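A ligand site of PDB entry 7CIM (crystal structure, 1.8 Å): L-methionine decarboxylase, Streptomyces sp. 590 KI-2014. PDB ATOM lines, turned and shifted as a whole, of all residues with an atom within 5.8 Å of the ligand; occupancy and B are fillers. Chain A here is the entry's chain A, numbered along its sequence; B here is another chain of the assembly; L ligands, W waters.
The side-chain amino group (NZ) of Lys 394 is bonded to a carbon (C8) of the ligand, 1.3 Å away. OD2 of Asp 336 lies within hydrogen-bond range of N1 of the ligand, 2.6 Å away. The backbone NH (N) of Ser 432 of chain B lies within hydrogen-bond range of an oxygen (O1) of the ligand (2.9 Å). O1 of the ligand sits at hydrogen-bond distance from OG of Ser 432 of chain B, 2.7 Å away. A ring nitrogen (NE2) of His 393 is in hydrogen-bond range of an oxygen (O2) of the ligand. An oxygen (O3) of the ligand sits at hydrogen-bond distance from the backbone NH (N) of Thr 139 (2.9 Å). The side-chain hydroxyl (OG1) of Thr 139 lies within hydrogen-bond range of an oxygen (O3) of the ligand (2.8 Å). N of Ser 138 lies within hydrogen-bond range of O2 of the ligand, 3.0 Å away. OG of Ser 391 is in hydrogen-bond range of O2 of the ligand (3.1 Å). O5 of the ligand is in hydrogen-bond range of OG1 of Thr 283.
The side-chain carboxylate (OD1) of Asp 336 sits at hydrogen-bond distance from the backbone NH (N) of Ala 338 (3.2 Å). OG of Ser 432 of chain B is in hydrogen-bond range of ND2 of Asn 85 of chain B, 2.8 Å away. The side-chain hydroxyl (OG1) of Thr 139 sits at hydrogen-bond distance from the backbone NH (N) of Gly 431 of chain B (3.3 Å). OG of Ser 138 lies within hydrogen-bond range of OG of Ser 391, 2.5 Å away. N of Ser 391 is in hydrogen-bond range of O of Ala 338, 2.9 Å away. A ring nitrogen (ND1) of His 195 is in hydrogen-bond range of the side-chain hydroxyl of Thr 283, at 3.2 Å. The backbone carbonyl oxygen (O) of Thr 283 sits at hydrogen-bond distance from the side-chain amide nitrogen (NE2) of Gln 64 (2.9 Å). N of Leu 87 of chain B sits at hydrogen-bond distance from OD1 of Asn 85 of chain B (3.1 Å).
Water W6 lies within hydrogen-bond range of O5 of the ligand (2.6 Å), O of Gly 281 (2.9 Å) and NE2 of Gln 64 (3.0 Å). Water W4 lies within hydrogen-bond range of the backbone carbonyl oxygen of Ser 432 of chain B, an oxygen (O3) of the ligand, the backbone NH of Gly 137 and the backbone NH of Gly 431 of chain B. Water W5 bridges N of Thr 283 and N of His 195. Water W3 lies within hydrogen-bond range of ND2 of Asn 279 (2.8 Å), OD2 of Asp 336 (2.8 Å) and N of His 195 (2.8 Å). Water W2 lies within hydrogen-bond range of ND2 of Asn 85 of chain B (2.9 Å) and OH of Tyr 96 of chain B (3.0 Å). Water W1 lies within hydrogen-bond range of N of Leu 339 (2.8 Å), O of Gly 281 (2.8 Å), N of Ala 338 (3.0 Å) and O of Asp 336 (3.2 Å).
Merely in contact with the ligand: His 195, Gly 137, Tyr 421 of chain B, Asn 142, Ala 338, Ser 197, Gly 281, Asn 85 of chain B, Ala 65, Gln 64, Leu 87 of chain B and Gly 431 of chain B. Hydrophobic or aromatic side chains that line the ligand: Ala 65, His 195, Ala 338, His 393 and Leu 87 of chain B. Of the 30 residues printed, 20 come within 4 Å of the ligand. The nearest printed residue that does not touch the ligand is Tyr 63 (4.1 Å).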
ATOM      1  N   TYR A  63     -16.640   3.024  -6.023  1.00  0.00           N
ATOM      2  CA  TYR A  63     -17.753   2.136  -6.345  1.00  0.00           C
ATOM      3  C   TYR A  63     -17.732   1.841  -7.834  1.00  0.00           C
ATOM      4  O   TYR A  63     -17.236   2.638  -8.638  1.00  0.00           O
ATOM      5  CB  TYR A  63     -19.102   2.759  -5.958  1.00  0.00           C
ATOM      6  CG  TYR A  63     -19.364   2.726  -4.465  1.00  0.00           C
ATOM      7  CD1 TYR A  63     -18.868   3.726  -3.641  1.00  0.00           C
ATOM      8  CD2 TYR A  63     -20.067   1.683  -3.879  1.00  0.00           C
ATOM      9  CE1 TYR A  63     -19.081   3.702  -2.285  1.00  0.00           C
ATOM     10  CE2 TYR A  63     -20.310   1.659  -2.513  1.00  0.00           C
ATOM     11  CZ  TYR A  63     -19.793   2.675  -1.716  1.00  0.00           C
ATOM     12  OH  TYR A  63     -19.982   2.672  -0.378  1.00  0.00           O
ATOM     13  N   GLN A  64     -18.309   0.704  -8.186  1.00  0.00           N
ATOM     14  CA  GLN A  64     -18.248   0.166  -9.532  1.00  0.00           C
ATOM     15  C   GLN A  64     -19.395   0.750 -10.363  1.00  0.00           C
ATOM     16  O   GLN A  64     -20.175   0.021 -10.956  1.00  0.00           O
ATOM     17  CB  GLN A  64     -18.239  -1.385  -9.532  1.00  0.00           C
ATOM     18  CG  GLN A  64     -19.333  -2.068  -8.696  1.00  0.00           C
ATOM     19  CD  GLN A  64     -18.899  -2.330  -7.263  1.00  0.00           C
ATOM     20  OE1 GLN A  64     -18.800  -1.401  -6.441  1.00  0.00           O
ATOM     21  NE2 GLN A  64     -18.613  -3.585  -6.942  1.00  0.00           N
ATOM     22  N   ALA A  65     -19.434   2.084 -10.438  1.00  0.00           N
ATOM     23  CA  ALA A  65     -20.489   2.803 -11.132  1.00  0.00           C
ATOM     24  C   ALA A  65     -19.864   3.901 -11.969  1.00  0.00           C
ATOM     25  O   ALA A  65     -19.284   4.822 -11.439  1.00  0.00           O
ATOM     26  CB  ALA A  65     -21.483   3.398 -10.141  1.00  0.00           C
ATOM     27  N   MET A 136     -35.138  -2.336 -11.205  1.00  0.00           N
ATOM     28  CA  MET A 136     -34.128  -2.129 -10.166  1.00  0.00           C
ATOM     29  C   MET A 136     -32.796  -2.456 -10.868  1.00  0.00           C
ATOM     30  O   MET A 136     -32.747  -2.617 -12.070  1.00  0.00           O
ATOM     31  CB  MET A 136     -34.311  -3.088  -8.961  1.00  0.00           C
ATOM     32  CG  MET A 136     -35.722  -3.289  -8.464  1.00  0.00           C
ATOM     33  SD  MET A 136     -35.834  -4.119  -6.857  1.00  0.00           S
ATOM     34  CE  MET A 136     -35.894  -5.865  -7.251  1.00  0.00           C
ATOM     35  N   GLY A 137     -31.712  -2.573 -10.112  1.00  0.00           N
ATOM     36  CA  GLY A 137     -30.465  -3.108 -10.654  1.00  0.00           C
ATOM     37  C   GLY A 137     -30.420  -4.625 -10.683  1.00  0.00           C
ATOM     38  O   GLY A 137     -31.472  -5.276 -10.707  1.00  0.00           O
ATOM     39  N   SER A 138     -29.199  -5.185 -10.651  1.00  0.00           N
ATOM     40  CA  SER A 138     -29.037  -6.634 -10.682  1.00  0.00           C
ATOM     41  C   SER A 138     -29.676  -7.384  -9.514  1.00  0.00           C
ATOM     42  O   SER A 138     -29.885  -8.562  -9.630  1.00  0.00           O
ATOM     43  CB  SER A 138     -27.552  -7.030 -10.759  1.00  0.00           C
ATOM     44  OG  SER A 138     -27.020  -6.732 -12.018  1.00  0.00           O
ATOM     45  N   THR A 139     -29.948  -6.730  -8.377  1.00  0.00           N
ATOM     46  CA  THR A 139     -30.751  -7.367  -7.342  1.00  0.00           C
ATOM     47  C   THR A 139     -32.008  -7.989  -7.977  1.00  0.00           C
ATOM     48  O   THR A 139     -32.298  -9.162  -7.721  1.00  0.00           O
ATOM     49  CB  THR A 139     -31.144  -6.415  -6.206  1.00  0.00           C
ATOM     50  OG1 THR A 139     -29.964  -5.983  -5.504  1.00  0.00           O
ATOM     51  CG2 THR A 139     -32.070  -7.109  -5.217  1.00  0.00           C
ATOM     52  N   GLU A 140     -32.722  -7.244  -8.815  1.00  0.00           N
ATOM     53  CA  GLU A 140     -33.897  -7.794  -9.523  1.00  0.00           C
ATOM     54  C   GLU A 140     -33.565  -9.007 -10.415  1.00  0.00           C
ATOM     55  O   GLU A 140     -34.324  -9.978 -10.454  1.00  0.00           O
ATOM     56  CB  GLU A 140     -34.634  -6.718 -10.354  1.00  0.00           C
ATOM     57  CG  GLU A 140     -35.976  -7.210 -10.926  1.00  0.00           C
ATOM     58  CD  GLU A 140     -36.664  -6.275 -11.918  1.00  0.00           C
ATOM     59  OE1 GLU A 140     -36.345  -5.073 -11.978  1.00  0.00           O
ATOM     60  OE2 GLU A 140     -37.514  -6.772 -12.684  1.00  0.00           O
ATOM     61  N   ASN A 142     -30.884 -11.100 -10.164  1.00  0.00           N
ATOM     62  CA  ASN A 142     -30.514 -12.227  -9.330  1.00  0.00           C
ATOM     63  C   ASN A 142     -31.737 -12.875  -8.650  1.00  0.00           C
ATOM     64  O   ASN A 142     -31.800 -14.092  -8.522  1.00  0.00           O
ATOM     65  CB  ASN A 142     -29.470 -11.801  -8.300  1.00  0.00           C
ATOM     66  CG  ASN A 142     -28.127 -11.479  -8.943  1.00  0.00           C
ATOM     67  OD1 ASN A 142     -27.826 -11.926 -10.047  1.00  0.00           O
ATOM     68  ND2 ASN A 142     -27.304 -10.727  -8.226  1.00  0.00           N
ATOM     69  N   HIS A 195     -22.222 -11.377  -3.582  1.00  0.00           N
ATOM     70  CA  HIS A 195     -22.853 -10.179  -3.074  1.00  0.00           C
ATOM     71  C   HIS A 195     -23.999 -10.526  -2.120  1.00  0.00           C
ATOM     72  O   HIS A 195     -24.691 -11.521  -2.310  1.00  0.00           O
ATOM     73  CB  HIS A 195     -23.348  -9.274  -4.224  1.00  0.00           C
ATOM     74  CG  HIS A 195     -23.793  -7.924  -3.771  1.00  0.00           C
ATOM     75  ND1 HIS A 195     -23.000  -7.101  -2.995  1.00  0.00           N
ATOM     76  CD2 HIS A 195     -24.961  -7.267  -3.947  1.00  0.00           C
ATOM     77  CE1 HIS A 195     -23.653  -5.982  -2.732  1.00  0.00           C
ATOM     78  NE2 HIS A 195     -24.845  -6.057  -3.305  1.00  0.00           N
ATOM     79  N   SER A 197     -26.896  -9.326  -1.772  1.00  0.00           N
ATOM     80  CA  SER A 197     -28.157  -9.495  -2.485  1.00  0.00           C
ATOM     81  C   SER A 197     -28.574 -10.953  -2.666  1.00  0.00           C
ATOM     82  O   SER A 197     -29.779 -11.253  -2.669  1.00  0.00           O
ATOM     83  CB  SER A 197     -28.098  -8.821  -3.863  1.00  0.00           C
ATOM     84  OG  SER A 197     -27.297  -9.570  -4.785  1.00  0.00           O
ATOM     85  N   ASN A 279     -19.786 -15.530  -9.866  1.00  0.00           N
ATOM     86  CA  ASN A 279     -19.553 -14.076  -9.895  1.00  0.00           C
ATOM     87  C   ASN A 279     -18.594 -13.685 -10.989  1.00  0.00           C
ATOM     88  O   ASN A 279     -17.439 -14.132 -10.984  1.00  0.00           O
ATOM     89  CB  ASN A 279     -18.994 -13.570  -8.546  1.00  0.00           C
ATOM     90  CG  ASN A 279     -19.778 -14.111  -7.364  1.00  0.00           C
ATOM     91  OD1 ASN A 279     -19.201 -14.752  -6.467  1.00  0.00           O
ATOM     92  ND2 ASN A 279     -21.086 -13.911  -7.375  1.00  0.00           N
ATOM     93  N   GLY A 281     -16.998 -10.545 -11.807  1.00  0.00           N
ATOM     94  CA  GLY A 281     -16.683  -9.209 -11.373  1.00  0.00           C
ATOM     95  C   GLY A 281     -17.276  -9.036  -9.984  1.00  0.00           C
ATOM     96  O   GLY A 281     -18.318  -8.380  -9.812  1.00  0.00           O
ATOM     97  N   SER A 282     -16.661  -9.678  -9.008  1.00  0.00           N
ATOM     98  CA  SER A 282     -17.203  -9.699  -7.641  1.00  0.00           C
ATOM     99  C   SER A 282     -17.173  -8.322  -6.999  1.00  0.00           C
ATOM    100  O   SER A 282     -16.393  -7.442  -7.386  1.00  0.00           O
ATOM    101  CB  SER A 282     -16.465 -10.745  -6.755  1.00  0.00           C
ATOM    102  OG  SER A 282     -15.125 -10.374  -6.520  1.00  0.00           O
ATOM    103  N   THR A 283     -18.001  -8.137  -5.982  1.00  0.00           N
ATOM    104  CA  THR A 283     -18.267  -6.808  -5.456  1.00  0.00           C
ATOM    105  C   THR A 283     -17.058  -6.107  -4.863  1.00  0.00           C
ATOM    106  O   THR A 283     -16.862  -4.919  -5.128  1.00  0.00           O
ATOM    107  CB  THR A 283     -19.382  -6.811  -4.403  1.00  0.00           C
ATOM    108  OG1 THR A 283     -20.489  -7.542  -4.926  1.00  0.00           O
ATOM    109  CG2 THR A 283     -19.830  -5.390  -4.120  1.00  0.00           C
ATOM    110  N   ASP A 336     -23.715 -14.065 -12.218  1.00  0.00           N
ATOM    111  CA  ASP A 336     -23.905 -12.746 -11.725  1.00  0.00           C
ATOM    112  C   ASP A 336     -22.804 -11.857 -12.323  1.00  0.00           C
ATOM    113  O   ASP A 336     -21.681 -11.706 -11.783  1.00  0.00           O
ATOM    114  CB  ASP A 336     -23.907 -12.694 -10.190  1.00  0.00           C
ATOM    115  CG  ASP A 336     -24.210 -11.312  -9.663  1.00  0.00           C
ATOM    116  OD1 ASP A 336     -24.433 -10.383 -10.469  1.00  0.00           O
ATOM    117  OD2 ASP A 336     -24.183 -11.121  -8.397  1.00  0.00           O
ATOM    118  N   ALA A 338     -23.273  -8.578 -12.856  1.00  0.00           N
ATOM    119  CA  ALA A 338     -23.769  -7.245 -12.562  1.00  0.00           C
ATOM    120  C   ALA A 338     -22.782  -6.241 -13.114  1.00  0.00           C
ATOM    121  O   ALA A 338     -23.164  -5.280 -13.810  1.00  0.00           O
ATOM    122  CB  ALA A 338     -23.891  -7.040 -11.065  1.00  0.00           C
ATOM    123  N   LEU A 339     -21.527  -6.468 -12.806  1.00  0.00           N
ATOM    124  CA  LEU A 339     -20.459  -5.643 -13.317  1.00  0.00           C
ATOM    125  C   LEU A 339     -19.877  -6.231 -14.605  1.00  0.00           C
ATOM    126  O   LEU A 339     -19.883  -5.576 -15.652  1.00  0.00           O
ATOM    127  CB  LEU A 339     -19.344  -5.491 -12.256  1.00  0.00           C
ATOM    128  CG  LEU A 339     -18.043  -4.781 -12.658  1.00  0.00           C
ATOM    129  CD1 LEU A 339     -18.300  -3.361 -13.134  1.00  0.00           C
ATOM    130  CD2 LEU A 339     -17.047  -4.763 -11.505  1.00  0.00           C
ATOM    131  N   SER A 391     -25.900  -5.168 -14.638  1.00  0.00           N
ATOM    132  CA  SER A 391     -26.354  -3.831 -14.211  1.00  0.00           C
ATOM    133  C   SER A 391     -25.887  -2.786 -15.210  1.00  0.00           C
ATOM    134  O   SER A 391     -24.709  -2.766 -15.530  1.00  0.00           O
ATOM    135  CB  SER A 391     -25.785  -3.490 -12.824  1.00  0.00           C
ATOM    136  OG  SER A 391     -26.227  -4.402 -11.848  1.00  0.00           O
ATOM    137  N   HIS A 393     -26.171   0.525 -14.807  1.00  0.00           N
ATOM    138  CA  HIS A 393     -25.567   1.575 -13.999  1.00  0.00           C
ATOM    139  C   HIS A 393     -24.160   1.288 -13.487  1.00  0.00           C
ATOM    140  O   HIS A 393     -23.595   2.156 -12.801  1.00  0.00           O
ATOM    141  CB  HIS A 393     -26.479   1.944 -12.840  1.00  0.00           C
ATOM    142  CG  HIS A 393     -26.812   0.804 -11.926  1.00  0.00           C
ATOM    143  ND1 HIS A 393     -26.483   0.787 -10.592  1.00  0.00           N
ATOM    144  CD2 HIS A 393     -27.433  -0.377 -12.161  1.00  0.00           C
ATOM    145  CE1 HIS A 393     -26.881  -0.341 -10.052  1.00  0.00           C
ATOM    146  NE2 HIS A 393     -27.463  -1.070 -10.981  1.00  0.00           N
ATOM    147  N   LYS A 394     -23.621   0.084 -13.716  1.00  0.00           N
ATOM    148  CA  LYS A 394     -22.252  -0.233 -13.339  1.00  0.00           C
ATOM    149  C   LYS A 394     -21.305   0.160 -14.499  1.00  0.00           C
ATOM    150  O   LYS A 394     -20.920   1.322 -14.588  1.00  0.00           O
ATOM    151  CB  LYS A 394     -22.113  -1.685 -12.818  1.00  0.00           C
ATOM    152  CG  LYS A 394     -22.856  -1.889 -11.482  1.00  0.00           C
ATOM    153  CD  LYS A 394     -22.580  -3.204 -10.714  1.00  0.00           C
ATOM    154  CE  LYS A 394     -23.589  -3.354  -9.551  1.00  0.00           C
ATOM    155  NZ  LYS A 394     -23.264  -4.058  -8.237  1.00  0.00           N
ATOM    156  N   PRO A 401     -30.676   2.834 -11.154  1.00  0.00           N
ATOM    157  CA  PRO A 401     -30.427   1.396 -11.348  1.00  0.00           C
ATOM    158  C   PRO A 401     -31.222   0.789 -12.499  1.00  0.00           C
ATOM    159  O   PRO A 401     -32.395   1.083 -12.670  1.00  0.00           O
ATOM    160  CB  PRO A 401     -30.821   0.796 -10.001  1.00  0.00           C
ATOM    161  CG  PRO A 401     -30.510   1.918  -9.017  1.00  0.00           C
ATOM    162  CD  PRO A 401     -31.037   3.128  -9.753  1.00  0.00           C
ATOM    163  N   CYS A 402     -30.543  -0.009 -13.321  1.00  0.00           N
ATOM    164  CA  CYS A 402     -31.209  -0.725 -14.410  1.00  0.00           C
ATOM    165  C   CYS A 402     -30.369  -1.942 -14.810  1.00  0.00           C
ATOM    166  O   CYS A 402     -29.376  -2.226 -14.188  1.00  0.00           O
ATOM    167  CB  CYS A 402     -31.382   0.226 -15.568  1.00  0.00           C
ATOM    168  SG  CYS A 402     -29.807   0.804 -16.249  1.00  0.00           S
ATOM    169  N   ASN B  85     -27.394   6.961  -6.495  1.00  0.00           N
ATOM    170  CA  ASN B  85     -27.653   5.617  -5.941  1.00  0.00           C
ATOM    171  C   ASN B  85     -27.962   5.719  -4.470  1.00  0.00           C
ATOM    172  O   ASN B  85     -27.094   6.141  -3.710  1.00  0.00           O
ATOM    173  CB  ASN B  85     -26.447   4.708  -6.228  1.00  0.00           C
ATOM    174  CG  ASN B  85     -26.779   3.228  -6.025  1.00  0.00           C
ATOM    175  OD1 ASN B  85     -27.634   2.864  -5.234  1.00  0.00           O
ATOM    176  ND2 ASN B  85     -26.080   2.369  -6.758  1.00  0.00           N
ATOM    177  N   LEU B  87     -28.516   3.386  -2.333  1.00  0.00           N
ATOM    178  CA  LEU B  87     -28.062   2.149  -1.698  1.00  0.00           C
ATOM    179  C   LEU B  87     -28.142   2.246  -0.191  1.00  0.00           C
ATOM    180  O   LEU B  87     -27.645   3.203   0.398  1.00  0.00           O
ATOM    181  CB  LEU B  87     -26.596   1.910  -2.095  1.00  0.00           C
ATOM    182  CG  LEU B  87     -25.922   0.649  -1.596  1.00  0.00           C
ATOM    183  CD1 LEU B  87     -26.641  -0.585  -2.119  1.00  0.00           C
ATOM    184  CD2 LEU B  87     -24.469   0.675  -2.040  1.00  0.00           C
ATOM    185  N   TYR B  96     -21.655   5.564  -0.622  1.00  0.00           N
ATOM    186  CA  TYR B  96     -21.909   6.068  -1.963  1.00  0.00           C
ATOM    187  C   TYR B  96     -22.448   7.499  -1.871  1.00  0.00           C
ATOM    188  O   TYR B  96     -23.670   7.708  -1.743  1.00  0.00           O
ATOM    189  CB  TYR B  96     -22.865   5.146  -2.705  1.00  0.00           C
ATOM    190  CG  TYR B  96     -22.930   5.396  -4.193  1.00  0.00           C
ATOM    191  CD1 TYR B  96     -23.632   6.507  -4.706  1.00  0.00           C
ATOM    192  CD2 TYR B  96     -22.326   4.535  -5.076  1.00  0.00           C
ATOM    193  CE1 TYR B  96     -23.706   6.712  -6.066  1.00  0.00           C
ATOM    194  CE2 TYR B  96     -22.398   4.721  -6.451  1.00  0.00           C
ATOM    195  CZ  TYR B  96     -23.065   5.826  -6.939  1.00  0.00           C
ATOM    196  OH  TYR B  96     -23.138   5.998  -8.296  1.00  0.00           O
ATOM    197  N   TYR B 421     -20.433  -4.988   3.932  1.00  0.00           N
ATOM    198  CA  TYR B 421     -19.986  -3.663   3.436  1.00  0.00           C
ATOM    199  C   TYR B 421     -21.134  -2.626   3.552  1.00  0.00           C
ATOM    200  O   TYR B 421     -22.204  -2.950   4.077  1.00  0.00           O
ATOM    201  CB  TYR B 421     -19.405  -3.778   2.002  1.00  0.00           C
ATOM    202  CG  TYR B 421     -20.350  -3.446   0.833  1.00  0.00           C
ATOM    203  CD1 TYR B 421     -21.646  -3.972   0.780  1.00  0.00           C
ATOM    204  CD2 TYR B 421     -19.922  -2.629  -0.221  1.00  0.00           C
ATOM    205  CE1 TYR B 421     -22.499  -3.666  -0.271  1.00  0.00           C
ATOM    206  CE2 TYR B 421     -20.772  -2.334  -1.291  1.00  0.00           C
ATOM    207  CZ  TYR B 421     -22.058  -2.853  -1.305  1.00  0.00           C
ATOM    208  OH  TYR B 421     -22.916  -2.573  -2.342  1.00  0.00           O
ATOM    209  N   ALA B 430     -34.862  -3.762  -2.976  1.00  0.00           N
ATOM    210  CA  ALA B 430     -33.807  -3.365  -3.933  1.00  0.00           C
ATOM    211  C   ALA B 430     -32.449  -3.225  -3.218  1.00  0.00           C
ATOM    212  O   ALA B 430     -32.417  -2.949  -2.005  1.00  0.00           O
ATOM    213  CB  ALA B 430     -34.175  -2.042  -4.591  1.00  0.00           C
ATOM    214  N   GLY B 431     -31.363  -3.408  -3.980  1.00  0.00           N
ATOM    215  CA  GLY B 431     -29.955  -3.257  -3.506  1.00  0.00           C
ATOM    216  C   GLY B 431     -29.483  -1.846  -3.808  1.00  0.00           C
ATOM    217  O   GLY B 431     -29.684  -0.951  -2.991  1.00  0.00           O
ATOM    218  N   SER B 432     -28.900  -1.609  -4.988  1.00  0.00           N
ATOM    219  CA  SER B 432     -28.858  -0.221  -5.520  1.00  0.00           C
ATOM    220  C   SER B 432     -30.308   0.264  -5.564  1.00  0.00           C
ATOM    221  O   SER B 432     -31.213  -0.523  -5.856  1.00  0.00           O
ATOM    222  CB  SER B 432     -28.252  -0.127  -6.942  1.00  0.00           C
ATOM    223  OG  SER B 432     -26.842  -0.315  -6.915  1.00  0.00           O
HETATM  224  C1  LIG L   1     -23.901  -5.864  -7.223  1.00  0.00           C
HETATM  225  C2  LIG L   1     -25.146  -6.511  -7.159  1.00  0.00           C
HETATM  226  C3  LIG L   1     -25.204  -7.888  -7.376  1.00  0.00           C
HETATM  227  N1  LIG L   1     -24.099  -8.598  -7.673  1.00  0.00           N
HETATM  228  C4  LIG L   1     -22.774  -6.651  -7.504  1.00  0.00           C
HETATM  229  O1  LIG L   1     -26.925  -2.988  -6.660  1.00  0.00           O
HETATM  230  P1  LIG L   1     -27.657  -3.625  -7.820  1.00  0.00           P
HETATM  231  O2  LIG L   1     -27.393  -3.247  -9.205  1.00  0.00           O
HETATM  232  O3  LIG L   1     -28.980  -4.170  -7.462  1.00  0.00           O
HETATM  233  O4  LIG L   1     -26.766  -4.976  -7.933  1.00  0.00           O
HETATM  234  C5  LIG L   1     -26.472  -5.774  -6.831  1.00  0.00           C
HETATM  235  C6  LIG L   1     -22.844  -8.029  -7.728  1.00  0.00           C
HETATM  236  C7  LIG L   1     -21.637  -8.870  -8.059  1.00  0.00           C
HETATM  237  O5  LIG L   1     -21.573  -6.043  -7.570  1.00  0.00           O
HETATM  238  C8  LIG L   1     -23.694  -4.488  -7.058  1.00  0.00           C
HETATM  239  N2  LIG L   1     -22.847  -3.986  -5.958  1.00  0.00           N
HETATM  240  C9  LIG L   1     -22.499  -2.585  -5.716  1.00  0.00           C
HETATM  241  C10 LIG L   1     -23.761  -1.766  -5.817  1.00  0.00           C
HETATM  242  C11 LIG L   1     -23.450  -0.274  -5.787  1.00  0.00           C
HETATM  243  S1  LIG L   1     -22.305   0.373  -7.087  1.00  0.00           S
HETATM  244  C12 LIG L   1     -23.341   0.426  -8.535  1.00  0.00           C
HETATM  245  O   HOH W   1     -20.637  -8.681 -11.396  1.00  0.00           O
HETATM  246  O   HOH W   2     -24.763   3.558  -9.057  1.00  0.00           O
HETATM  247  O   HOH W   3     -22.375 -11.687  -6.387  1.00  0.00           O
HETATM  248  O   HOH W   4     -31.367  -2.806  -7.219  1.00  0.00           O
HETATM  249  O   HOH W   5     -19.761 -10.571  -5.868  1.00  0.00           O
HETATM  250  O   HOH W   6     -19.294  -5.873  -8.821  1.00  0.00           O
